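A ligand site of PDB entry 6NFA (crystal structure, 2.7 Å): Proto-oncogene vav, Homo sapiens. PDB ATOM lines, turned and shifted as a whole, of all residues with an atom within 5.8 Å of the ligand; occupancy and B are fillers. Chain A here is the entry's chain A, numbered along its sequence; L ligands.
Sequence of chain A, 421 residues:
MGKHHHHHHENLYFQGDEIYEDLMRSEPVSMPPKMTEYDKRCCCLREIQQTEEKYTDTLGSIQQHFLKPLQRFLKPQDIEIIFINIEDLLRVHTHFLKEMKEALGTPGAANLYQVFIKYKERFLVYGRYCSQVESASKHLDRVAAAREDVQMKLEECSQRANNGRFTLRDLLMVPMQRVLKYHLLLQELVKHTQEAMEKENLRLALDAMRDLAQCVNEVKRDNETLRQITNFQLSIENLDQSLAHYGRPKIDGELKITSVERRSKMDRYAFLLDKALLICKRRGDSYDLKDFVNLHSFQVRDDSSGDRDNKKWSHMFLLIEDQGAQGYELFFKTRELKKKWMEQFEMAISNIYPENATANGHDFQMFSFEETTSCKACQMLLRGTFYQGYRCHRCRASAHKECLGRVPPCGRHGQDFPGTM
N of Leu 382 lies within hydrogen-bond range of O of Thr 373, 3.0 Å away. The side-chain hydroxyl (OG1) of Thr 373 is in hydrogen-bond range of the backbone carbonyl oxygen (O) of Glu 371, at 3.0 Å. The backbone carbonyl oxygen (O) of Gly 384 sits at hydrogen-bond distance from the side-chain amide nitrogen (NE2) of Gln 388. The side-chain sulfur of Cys 215 lies within hydrogen-bond range of the guanidinium group of Arg 383, at 3.6 Å. OE1 of Gln 388 lies within hydrogen-bond range of N of Phe 369 (2.8 Å).
Residues that only touch the ligand: Glu 371 (3.4 Å), Cys 215 (3.4 Å), Leu 124 (3.5 Å), Val 219 (3.5 Å), Phe 123 (3.5 Å), Tyr 126 (3.5 Å), Thr 385 (3.5 Å), Gly 127 (3.6 Å), Arg 128 (3.6 Å), Leu 381 (3.7 Å), Gln 388 (3.7 Å), Val 216 (3.8 Å), Arg 383 (3.8 Å), Leu 212 (3.9 Å) and Glu 370 (3.95 Å). Hydrophobic or aromatic side chains that line the ligand: Tyr 126, Leu 212, Val 216, Val 219 and Leu 381. 19 residues have an atom within 4 Å of the ligand: Phe 123, Leu 124, Tyr 126, Gly 127, Arg 128, Leu 212, Cys 215, Val 216, Val 219, Glu 370, Glu 371, Thr 372, Thr 373, Leu 381, Leu 382, Arg 383, Gly 384, Thr 385 and Gln 388. The nearest printed residue that does not touch the ligand is Phe 369 (4.03 Å).
OG1 of Thr 372 is in hydrogen-bond range of N2 of the ligand (2.8 Å). O of Leu 382 sits at hydrogen-bond distance from O1 of the ligand (2.9 Å). N of Thr 373 is in hydrogen-bond range of O1 of the ligand, at 2.9 Å. N of Gly 384 is in hydrogen-bond range of N3 of the ligand (3.1 Å). O of Gly 384 lies within hydrogen-bond range of N4 of the ligand (3.1 Å).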
ATOM      1  N   PHE A 123      -4.462 -21.287 -17.916  1.00  0.00           N
ATOM      2  CA  PHE A 123      -3.182 -21.977 -17.704  1.00  0.00           C
ATOM      3  C   PHE A 123      -2.181 -21.209 -16.810  1.00  0.00           C
ATOM      4  O   PHE A 123      -0.987 -21.540 -16.738  1.00  0.00           O
ATOM      5  CB  PHE A 123      -2.539 -22.341 -19.054  1.00  0.00           C
ATOM      6  CG  PHE A 123      -3.163 -23.522 -19.767  1.00  0.00           C
ATOM      7  CD1 PHE A 123      -3.886 -24.477 -19.063  1.00  0.00           C
ATOM      8  CD2 PHE A 123      -2.991 -23.699 -21.139  1.00  0.00           C
ATOM      9  CE1 PHE A 123      -4.463 -25.576 -19.725  1.00  0.00           C
ATOM     10  CE2 PHE A 123      -3.555 -24.802 -21.795  1.00  0.00           C
ATOM     11  CZ  PHE A 123      -4.292 -25.728 -21.080  1.00  0.00           C
ATOM     12  N   LEU A 124      -2.681 -20.170 -16.137  1.00  0.00           N
ATOM     13  CA  LEU A 124      -1.923 -19.325 -15.235  1.00  0.00           C
ATOM     14  C   LEU A 124      -1.550 -20.075 -13.941  1.00  0.00           C
ATOM     15  O   LEU A 124      -0.575 -19.731 -13.260  1.00  0.00           O
ATOM     16  CB  LEU A 124      -2.785 -18.101 -14.920  1.00  0.00           C
ATOM     17  CG  LEU A 124      -2.185 -16.758 -15.210  1.00  0.00           C
ATOM     18  CD1 LEU A 124      -1.795 -16.607 -16.712  1.00  0.00           C
ATOM     19  CD2 LEU A 124      -3.118 -15.677 -14.755  1.00  0.00           C
ATOM     20  N   VAL A 125      -2.369 -21.093 -13.627  1.00  0.00           N
ATOM     21  CA  VAL A 125      -2.252 -22.025 -12.510  1.00  0.00           C
ATOM     22  C   VAL A 125      -0.873 -22.717 -12.552  1.00  0.00           C
ATOM     23  O   VAL A 125      -0.341 -23.067 -11.502  1.00  0.00           O
ATOM     24  CB  VAL A 125      -3.470 -22.996 -12.565  1.00  0.00           C
ATOM     25  CG1 VAL A 125      -3.387 -24.063 -11.487  1.00  0.00           C
ATOM     26  CG2 VAL A 125      -4.783 -22.231 -12.431  1.00  0.00           C
ATOM     27  N   TYR A 126      -0.280 -22.837 -13.747  1.00  0.00           N
ATOM     28  CA  TYR A 126       1.053 -23.364 -14.009  1.00  0.00           C
ATOM     29  C   TYR A 126       2.187 -22.540 -13.376  1.00  0.00           C
ATOM     30  O   TYR A 126       3.319 -23.036 -13.277  1.00  0.00           O
ATOM     31  CB  TYR A 126       1.312 -23.415 -15.511  1.00  0.00           C
ATOM     32  CG  TYR A 126       0.941 -24.733 -16.140  1.00  0.00           C
ATOM     33  CD1 TYR A 126       1.852 -25.778 -16.202  1.00  0.00           C
ATOM     34  CD2 TYR A 126      -0.329 -24.928 -16.668  1.00  0.00           C
ATOM     35  CE1 TYR A 126       1.501 -27.003 -16.766  1.00  0.00           C
ATOM     36  CE2 TYR A 126      -0.686 -26.151 -17.253  1.00  0.00           C
ATOM     37  CZ  TYR A 126       0.237 -27.174 -17.295  1.00  0.00           C
ATOM     38  OH  TYR A 126      -0.084 -28.373 -17.875  1.00  0.00           O
ATOM     39  N   GLY A 127       1.910 -21.280 -13.024  1.00  0.00           N
ATOM     40  CA  GLY A 127       2.886 -20.390 -12.424  1.00  0.00           C
ATOM     41  C   GLY A 127       3.462 -20.945 -11.137  1.00  0.00           C
ATOM     42  O   GLY A 127       4.680 -21.100 -10.997  1.00  0.00           O
ATOM     43  N   ARG A 128       2.539 -21.297 -10.211  1.00  0.00           N
ATOM     44  CA  ARG A 128       2.802 -21.934  -8.924  1.00  0.00           C
ATOM     45  C   ARG A 128       3.582 -23.261  -9.183  1.00  0.00           C
ATOM     46  O   ARG A 128       4.614 -23.487  -8.552  1.00  0.00           O
ATOM     47  CB  ARG A 128       1.461 -22.231  -8.244  1.00  0.00           C
ATOM     48  CG  ARG A 128       1.552 -22.434  -6.754  1.00  0.00           C
ATOM     49  CD  ARG A 128       0.172 -22.698  -6.187  1.00  0.00           C
ATOM     50  NE  ARG A 128       0.241 -23.651  -5.079  1.00  0.00           N
ATOM     51  CZ  ARG A 128      -0.787 -24.383  -4.659  1.00  0.00           C
ATOM     52  NH1 ARG A 128      -1.968 -24.303  -5.249  1.00  0.00           N
ATOM     53  NH2 ARG A 128      -0.620 -25.229  -3.645  1.00  0.00           N
ATOM     54  N   CYS A 130       5.410 -24.306 -11.976  1.00  0.00           N
ATOM     55  CA  CYS A 130       6.706 -24.037 -12.565  1.00  0.00           C
ATOM     56  C   CYS A 130       7.732 -23.568 -11.536  1.00  0.00           C
ATOM     57  O   CYS A 130       8.895 -23.975 -11.605  1.00  0.00           O
ATOM     58  CB  CYS A 130       6.571 -23.033 -13.710  1.00  0.00           C
ATOM     59  SG  CYS A 130       8.080 -22.829 -14.694  1.00  0.00           S
ATOM     60  N   SER A 131       7.307 -22.687 -10.614  1.00  0.00           N
ATOM     61  CA  SER A 131       8.149 -22.144  -9.555  1.00  0.00           C
ATOM     62  C   SER A 131       8.582 -23.182  -8.519  1.00  0.00           C
ATOM     63  O   SER A 131       9.744 -23.164  -8.105  1.00  0.00           O
ATOM     64  CB  SER A 131       7.477 -20.954  -8.887  1.00  0.00           C
ATOM     65  OG  SER A 131       8.383 -20.259  -8.052  1.00  0.00           O
ATOM     66  N   MET A 176       5.594 -29.587 -17.339  1.00  0.00           N
ATOM     67  CA  MET A 176       6.473 -28.529 -17.809  1.00  0.00           C
ATOM     68  C   MET A 176       6.924 -28.735 -19.242  1.00  0.00           C
ATOM     69  O   MET A 176       7.003 -27.767 -20.000  1.00  0.00           O
ATOM     70  CB  MET A 176       7.665 -28.343 -16.861  1.00  0.00           C
ATOM     71  CG  MET A 176       7.286 -27.640 -15.574  1.00  0.00           C
ATOM     72  SD  MET A 176       6.690 -25.960 -15.912  1.00  0.00           S
ATOM     73  CE  MET A 176       5.049 -26.070 -15.341  1.00  0.00           C
ATOM     74  N   VAL A 179       3.705 -27.833 -21.605  1.00  0.00           N
ATOM     75  CA  VAL A 179       3.408 -26.408 -21.868  1.00  0.00           C
ATOM     76  C   VAL A 179       4.333 -25.819 -22.935  1.00  0.00           C
ATOM     77  O   VAL A 179       3.868 -25.012 -23.736  1.00  0.00           O
ATOM     78  CB  VAL A 179       3.335 -25.500 -20.625  1.00  0.00           C
ATOM     79  CG1 VAL A 179       1.962 -25.586 -19.965  1.00  0.00           C
ATOM     80  CG2 VAL A 179       4.451 -25.790 -19.635  1.00  0.00           C
ATOM     81  N   LEU A 212       3.057 -18.299 -23.484  1.00  0.00           N
ATOM     82  CA  LEU A 212       2.974 -19.288 -22.413  1.00  0.00           C
ATOM     83  C   LEU A 212       4.353 -19.920 -22.213  1.00  0.00           C
ATOM     84  O   LEU A 212       4.756 -20.124 -21.069  1.00  0.00           O
ATOM     85  CB  LEU A 212       1.934 -20.351 -22.779  1.00  0.00           C
ATOM     86  CG  LEU A 212       1.074 -20.910 -21.641  1.00  0.00           C
ATOM     87  CD1 LEU A 212       0.119 -19.859 -21.098  1.00  0.00           C
ATOM     88  CD2 LEU A 212       0.258 -22.094 -22.124  1.00  0.00           C
ATOM     89  N   CYS A 215       6.566 -17.412 -20.390  1.00  0.00           N
ATOM     90  CA  CYS A 215       6.182 -17.389 -18.983  1.00  0.00           C
ATOM     91  C   CYS A 215       6.954 -18.416 -18.165  1.00  0.00           C
ATOM     92  O   CYS A 215       7.232 -18.169 -16.995  1.00  0.00           O
ATOM     93  CB  CYS A 215       4.687 -17.585 -18.831  1.00  0.00           C
ATOM     94  SG  CYS A 215       3.694 -16.190 -19.387  1.00  0.00           S
ATOM     95  N   VAL A 216       7.294 -19.555 -18.782  1.00  0.00           N
ATOM     96  CA  VAL A 216       8.062 -20.623 -18.148  1.00  0.00           C
ATOM     97  C   VAL A 216       9.486 -20.139 -17.958  1.00  0.00           C
ATOM     98  O   VAL A 216      10.037 -20.244 -16.862  1.00  0.00           O
ATOM     99  CB  VAL A 216       7.987 -21.944 -18.973  1.00  0.00           C
ATOM    100  CG1 VAL A 216       8.920 -23.011 -18.412  1.00  0.00           C
ATOM    101  CG2 VAL A 216       6.554 -22.461 -19.031  1.00  0.00           C
ATOM    102  N   GLU A 218      10.714 -17.045 -17.854  1.00  0.00           N
ATOM    103  CA  GLU A 218      10.790 -15.970 -16.861  1.00  0.00           C
ATOM    104  C   GLU A 218      10.764 -16.506 -15.443  1.00  0.00           C
ATOM    105  O   GLU A 218      11.398 -15.921 -14.576  1.00  0.00           O
ATOM    106  CB  GLU A 218       9.667 -14.938 -17.067  1.00  0.00           C
ATOM    107  CG  GLU A 218       9.734 -14.169 -18.385  1.00  0.00           C
ATOM    108  CD  GLU A 218      11.035 -13.460 -18.702  1.00  0.00           C
ATOM    109  OE1 GLU A 218      11.521 -12.671 -17.863  1.00  0.00           O
ATOM    110  OE2 GLU A 218      11.553 -13.685 -19.820  1.00  0.00           O
ATOM    111  N   VAL A 219      10.053 -17.610 -15.196  1.00  0.00           N
ATOM    112  CA  VAL A 219       9.982 -18.212 -13.862  1.00  0.00           C
ATOM    113  C   VAL A 219      11.287 -18.952 -13.534  1.00  0.00           C
ATOM    114  O   VAL A 219      11.822 -18.787 -12.441  1.00  0.00           O
ATOM    115  CB  VAL A 219       8.697 -19.067 -13.652  1.00  0.00           C
ATOM    116  CG1 VAL A 219       8.789 -19.913 -12.386  1.00  0.00           C
ATOM    117  CG2 VAL A 219       7.470 -18.166 -13.601  1.00  0.00           C
ATOM    118  N   PHE A 369       6.571  -7.890  -7.591  1.00  0.00           N
ATOM    119  CA  PHE A 369       5.171  -8.231  -7.321  1.00  0.00           C
ATOM    120  C   PHE A 369       5.008  -9.628  -6.698  1.00  0.00           C
ATOM    121  O   PHE A 369       5.493 -10.601  -7.260  1.00  0.00           O
ATOM    122  CB  PHE A 369       4.361  -8.117  -8.638  1.00  0.00           C
ATOM    123  CG  PHE A 369       4.410  -6.742  -9.265  1.00  0.00           C
ATOM    124  CD1 PHE A 369       5.445  -6.384 -10.117  1.00  0.00           C
ATOM    125  CD2 PHE A 369       3.430  -5.795  -8.968  1.00  0.00           C
ATOM    126  CE1 PHE A 369       5.503  -5.093 -10.668  1.00  0.00           C
ATOM    127  CE2 PHE A 369       3.483  -4.508  -9.527  1.00  0.00           C
ATOM    128  CZ  PHE A 369       4.524  -4.177 -10.372  1.00  0.00           C
ATOM    129  N   GLU A 370       4.348  -9.702  -5.536  1.00  0.00           N
ATOM    130  CA  GLU A 370       4.071 -10.939  -4.809  1.00  0.00           C
ATOM    131  C   GLU A 370       2.940 -11.727  -5.483  1.00  0.00           C
ATOM    132  O   GLU A 370       3.059 -12.946  -5.682  1.00  0.00           O
ATOM    133  CB  GLU A 370       3.669 -10.661  -3.334  1.00  0.00           C
ATOM    134  CG  GLU A 370       4.773 -10.127  -2.433  1.00  0.00           C
ATOM    135  CD  GLU A 370       4.642 -10.342  -0.929  1.00  0.00           C
ATOM    136  OE1 GLU A 370       5.574  -9.940  -0.203  1.00  0.00           O
ATOM    137  OE2 GLU A 370       3.622 -10.932  -0.479  1.00  0.00           O
ATOM    138  N   GLU A 371       1.842 -11.033  -5.805  1.00  0.00           N
ATOM    139  CA  GLU A 371       0.663 -11.643  -6.426  1.00  0.00           C
ATOM    140  C   GLU A 371       0.647 -11.456  -7.935  1.00  0.00           C
ATOM    141  O   GLU A 371       1.386 -10.611  -8.445  1.00  0.00           O
ATOM    142  CB  GLU A 371      -0.634 -11.124  -5.769  1.00  0.00           C
ATOM    143  CG  GLU A 371      -0.926  -9.645  -5.993  1.00  0.00           C
ATOM    144  CD  GLU A 371      -2.160  -9.117  -5.293  1.00  0.00           C
ATOM    145  OE1 GLU A 371      -3.157  -8.839  -5.993  1.00  0.00           O
ATOM    146  OE2 GLU A 371      -2.135  -8.995  -4.045  1.00  0.00           O
ATOM    147  N   THR A 372      -0.200 -12.244  -8.648  1.00  0.00           N
ATOM    148  CA  THR A 372      -0.362 -12.170 -10.106  1.00  0.00           C
ATOM    149  C   THR A 372      -0.882 -10.786 -10.482  1.00  0.00           C
ATOM    150  O   THR A 372      -1.834 -10.296  -9.855  1.00  0.00           O
ATOM    151  CB  THR A 372      -1.175 -13.368 -10.585  1.00  0.00           C
ATOM    152  OG1 THR A 372      -0.400 -14.530 -10.324  1.00  0.00           O
ATOM    153  CG2 THR A 372      -1.492 -13.312 -12.058  1.00  0.00           C
ATOM    154  N   THR A 373      -0.176 -10.114 -11.408  1.00  0.00           N
ATOM    155  CA  THR A 373      -0.471  -8.731 -11.796  1.00  0.00           C
ATOM    156  C   THR A 373      -0.421  -8.524 -13.319  1.00  0.00           C
ATOM    157  O   THR A 373       0.380  -9.153 -14.007  1.00  0.00           O
ATOM    158  CB  THR A 373       0.472  -7.794 -11.015  1.00  0.00           C
ATOM    159  OG1 THR A 373       0.344  -8.055  -9.622  1.00  0.00           O
ATOM    160  CG2 THR A 373       0.214  -6.332 -11.256  1.00  0.00           C
ATOM    161  N   SER A 374      -1.278  -7.603 -13.813  1.00  0.00           N
ATOM    162  CA  SER A 374      -1.370  -7.216 -15.208  1.00  0.00           C
ATOM    163  C   SER A 374      -0.833  -5.804 -15.419  1.00  0.00           C
ATOM    164  O   SER A 374      -0.881  -4.986 -14.511  1.00  0.00           O
ATOM    165  CB  SER A 374      -2.821  -7.294 -15.685  1.00  0.00           C
ATOM    166  OG  SER A 374      -3.271  -8.627 -15.650  1.00  0.00           O
ATOM    167  N   LEU A 381       0.102  -9.934 -18.505  1.00  0.00           N
ATOM    168  CA  LEU A 381       0.786 -10.371 -17.272  1.00  0.00           C
ATOM    169  C   LEU A 381       2.214  -9.855 -17.147  1.00  0.00           C
ATOM    170  O   LEU A 381       2.964  -9.856 -18.139  1.00  0.00           O
ATOM    171  CB  LEU A 381       0.816 -11.929 -17.258  1.00  0.00           C
ATOM    172  CG  LEU A 381       1.577 -12.647 -16.135  1.00  0.00           C
ATOM    173  CD1 LEU A 381       0.783 -12.653 -14.821  1.00  0.00           C
ATOM    174  CD2 LEU A 381       2.029 -14.052 -16.562  1.00  0.00           C
ATOM    175  N   LEU A 382       2.607  -9.464 -15.919  1.00  0.00           N
ATOM    176  CA  LEU A 382       3.983  -9.099 -15.577  1.00  0.00           C
ATOM    177  C   LEU A 382       4.610 -10.456 -15.193  1.00  0.00           C
ATOM    178  O   LEU A 382       4.350 -10.997 -14.122  1.00  0.00           O
ATOM    179  CB  LEU A 382       3.993  -8.092 -14.414  1.00  0.00           C
ATOM    180  CG  LEU A 382       3.717  -6.633 -14.817  1.00  0.00           C
ATOM    181  CD1 LEU A 382       3.154  -5.863 -13.673  1.00  0.00           C
ATOM    182  CD2 LEU A 382       4.979  -5.942 -15.240  1.00  0.00           C
ATOM    183  N   ARG A 383       5.292 -11.071 -16.135  1.00  0.00           N
ATOM    184  CA  ARG A 383       5.832 -12.424 -16.010  1.00  0.00           C
ATOM    185  C   ARG A 383       6.981 -12.555 -15.039  1.00  0.00           C
ATOM    186  O   ARG A 383       7.824 -11.648 -14.936  1.00  0.00           O
ATOM    187  CB  ARG A 383       6.302 -12.934 -17.392  1.00  0.00           C
ATOM    188  CG  ARG A 383       5.238 -12.942 -18.480  1.00  0.00           C
ATOM    189  CD  ARG A 383       5.910 -13.204 -19.801  1.00  0.00           C
ATOM    190  NE  ARG A 383       4.972 -13.165 -20.915  1.00  0.00           N
ATOM    191  CZ  ARG A 383       5.340 -12.991 -22.185  1.00  0.00           C
ATOM    192  NH1 ARG A 383       6.618 -12.812 -22.488  1.00  0.00           N
ATOM    193  NH2 ARG A 383       4.425 -12.972 -23.144  1.00  0.00           N
ATOM    194  N   GLY A 384       7.080 -13.729 -14.398  1.00  0.00           N
ATOM    195  CA  GLY A 384       8.143 -14.024 -13.471  1.00  0.00           C
ATOM    196  C   GLY A 384       7.783 -13.850 -12.011  1.00  0.00           C
ATOM    197  O   GLY A 384       6.644 -13.512 -11.668  1.00  0.00           O
ATOM    198  N   THR A 385       8.788 -14.077 -11.147  1.00  0.00           N
ATOM    199  CA  THR A 385       8.672 -14.081  -9.681  1.00  0.00           C
ATOM    200  C   THR A 385       9.524 -13.016  -8.964  1.00  0.00           C
ATOM    201  O   THR A 385       9.487 -12.937  -7.747  1.00  0.00           O
ATOM    202  CB  THR A 385       9.087 -15.469  -9.171  1.00  0.00           C
ATOM    203  OG1 THR A 385      10.378 -15.780  -9.688  1.00  0.00           O
ATOM    204  CG2 THR A 385       8.130 -16.559  -9.582  1.00  0.00           C
ATOM    205  N   GLN A 388       9.567  -8.010 -11.915  1.00  0.00           N
ATOM    206  CA  GLN A 388       8.852  -8.245 -13.164  1.00  0.00           C
ATOM    207  C   GLN A 388       8.548  -6.987 -13.977  1.00  0.00           C
ATOM    208  O   GLN A 388       8.376  -7.086 -15.199  1.00  0.00           O
ATOM    209  CB  GLN A 388       7.555  -9.023 -12.861  1.00  0.00           C
ATOM    210  CG  GLN A 388       7.781 -10.246 -11.971  1.00  0.00           C
ATOM    211  CD  GLN A 388       7.433 -10.020 -10.525  1.00  0.00           C
ATOM    212  OE1 GLN A 388       7.639  -8.940  -9.987  1.00  0.00           O
ATOM    213  NE2 GLN A 388       6.995 -11.055  -9.818  1.00  0.00           N
HETATM  214  C1  LIG L   1       3.461 -15.627 -13.496  1.00  0.00           C
HETATM  215  C2  LIG L   1       1.662 -17.101 -13.452  1.00  0.00           C
HETATM  216  C3  LIG L   1       3.251 -13.073 -10.690  1.00  0.00           C
HETATM  217  C4  LIG L   1       3.459 -11.548 -10.912  1.00  0.00           C
HETATM  218  C5  LIG L   1       4.019 -13.638  -9.452  1.00  0.00           C
HETATM  219  C6  LIG L   1       2.147 -18.666 -16.349  1.00  0.00           C
HETATM  220  C7  LIG L   1       1.962 -19.776 -17.180  1.00  0.00           C
HETATM  221  C8  LIG L   1       2.977 -20.737 -17.344  1.00  0.00           C
HETATM  222  C9  LIG L   1       4.213 -20.593 -16.673  1.00  0.00           C
HETATM  223  C10 LIG L   1       4.391 -19.506 -15.803  1.00  0.00           C
HETATM  224  C11 LIG L   1       2.743 -21.921 -18.291  1.00  0.00           C
HETATM  225  C12 LIG L   1       3.842 -15.173  -9.347  1.00  0.00           C
HETATM  226  C13 LIG L   1       2.760 -15.736  -8.638  1.00  0.00           C
HETATM  227  C14 LIG L   1       3.428 -17.937  -9.237  1.00  0.00           C
HETATM  228  C15 LIG L   1       4.532 -17.439  -9.961  1.00  0.00           C
HETATM  229  C16 LIG L   1       4.725 -16.046 -10.022  1.00  0.00           C
HETATM  230  N1  LIG L   1       2.843 -16.718 -13.906  1.00  0.00           N
HETATM  231  C17 LIG L   1       1.044 -16.334 -12.535  1.00  0.00           C
HETATM  232  N2  LIG L   1       1.718 -15.150 -12.033  1.00  0.00           N
HETATM  233  C18 LIG L   1       2.885 -14.754 -12.445  1.00  0.00           C
HETATM  234  N3  LIG L   1       4.563 -15.493 -14.080  1.00  0.00           N
HETATM  235  C19 LIG L   1       4.749 -16.568 -15.021  1.00  0.00           C
HETATM  236  C20 LIG L   1       3.633 -17.310 -14.790  1.00  0.00           C
HETATM  237  C21 LIG L   1       3.354 -18.547 -15.624  1.00  0.00           C
HETATM  238  N4  LIG L   1       3.569 -13.738 -11.974  1.00  0.00           N
HETATM  239  O1  LIG L   1       2.516 -11.058 -11.892  1.00  0.00           O
HETATM  240  N5  LIG L   1       2.568 -17.083  -8.607  1.00  0.00           N
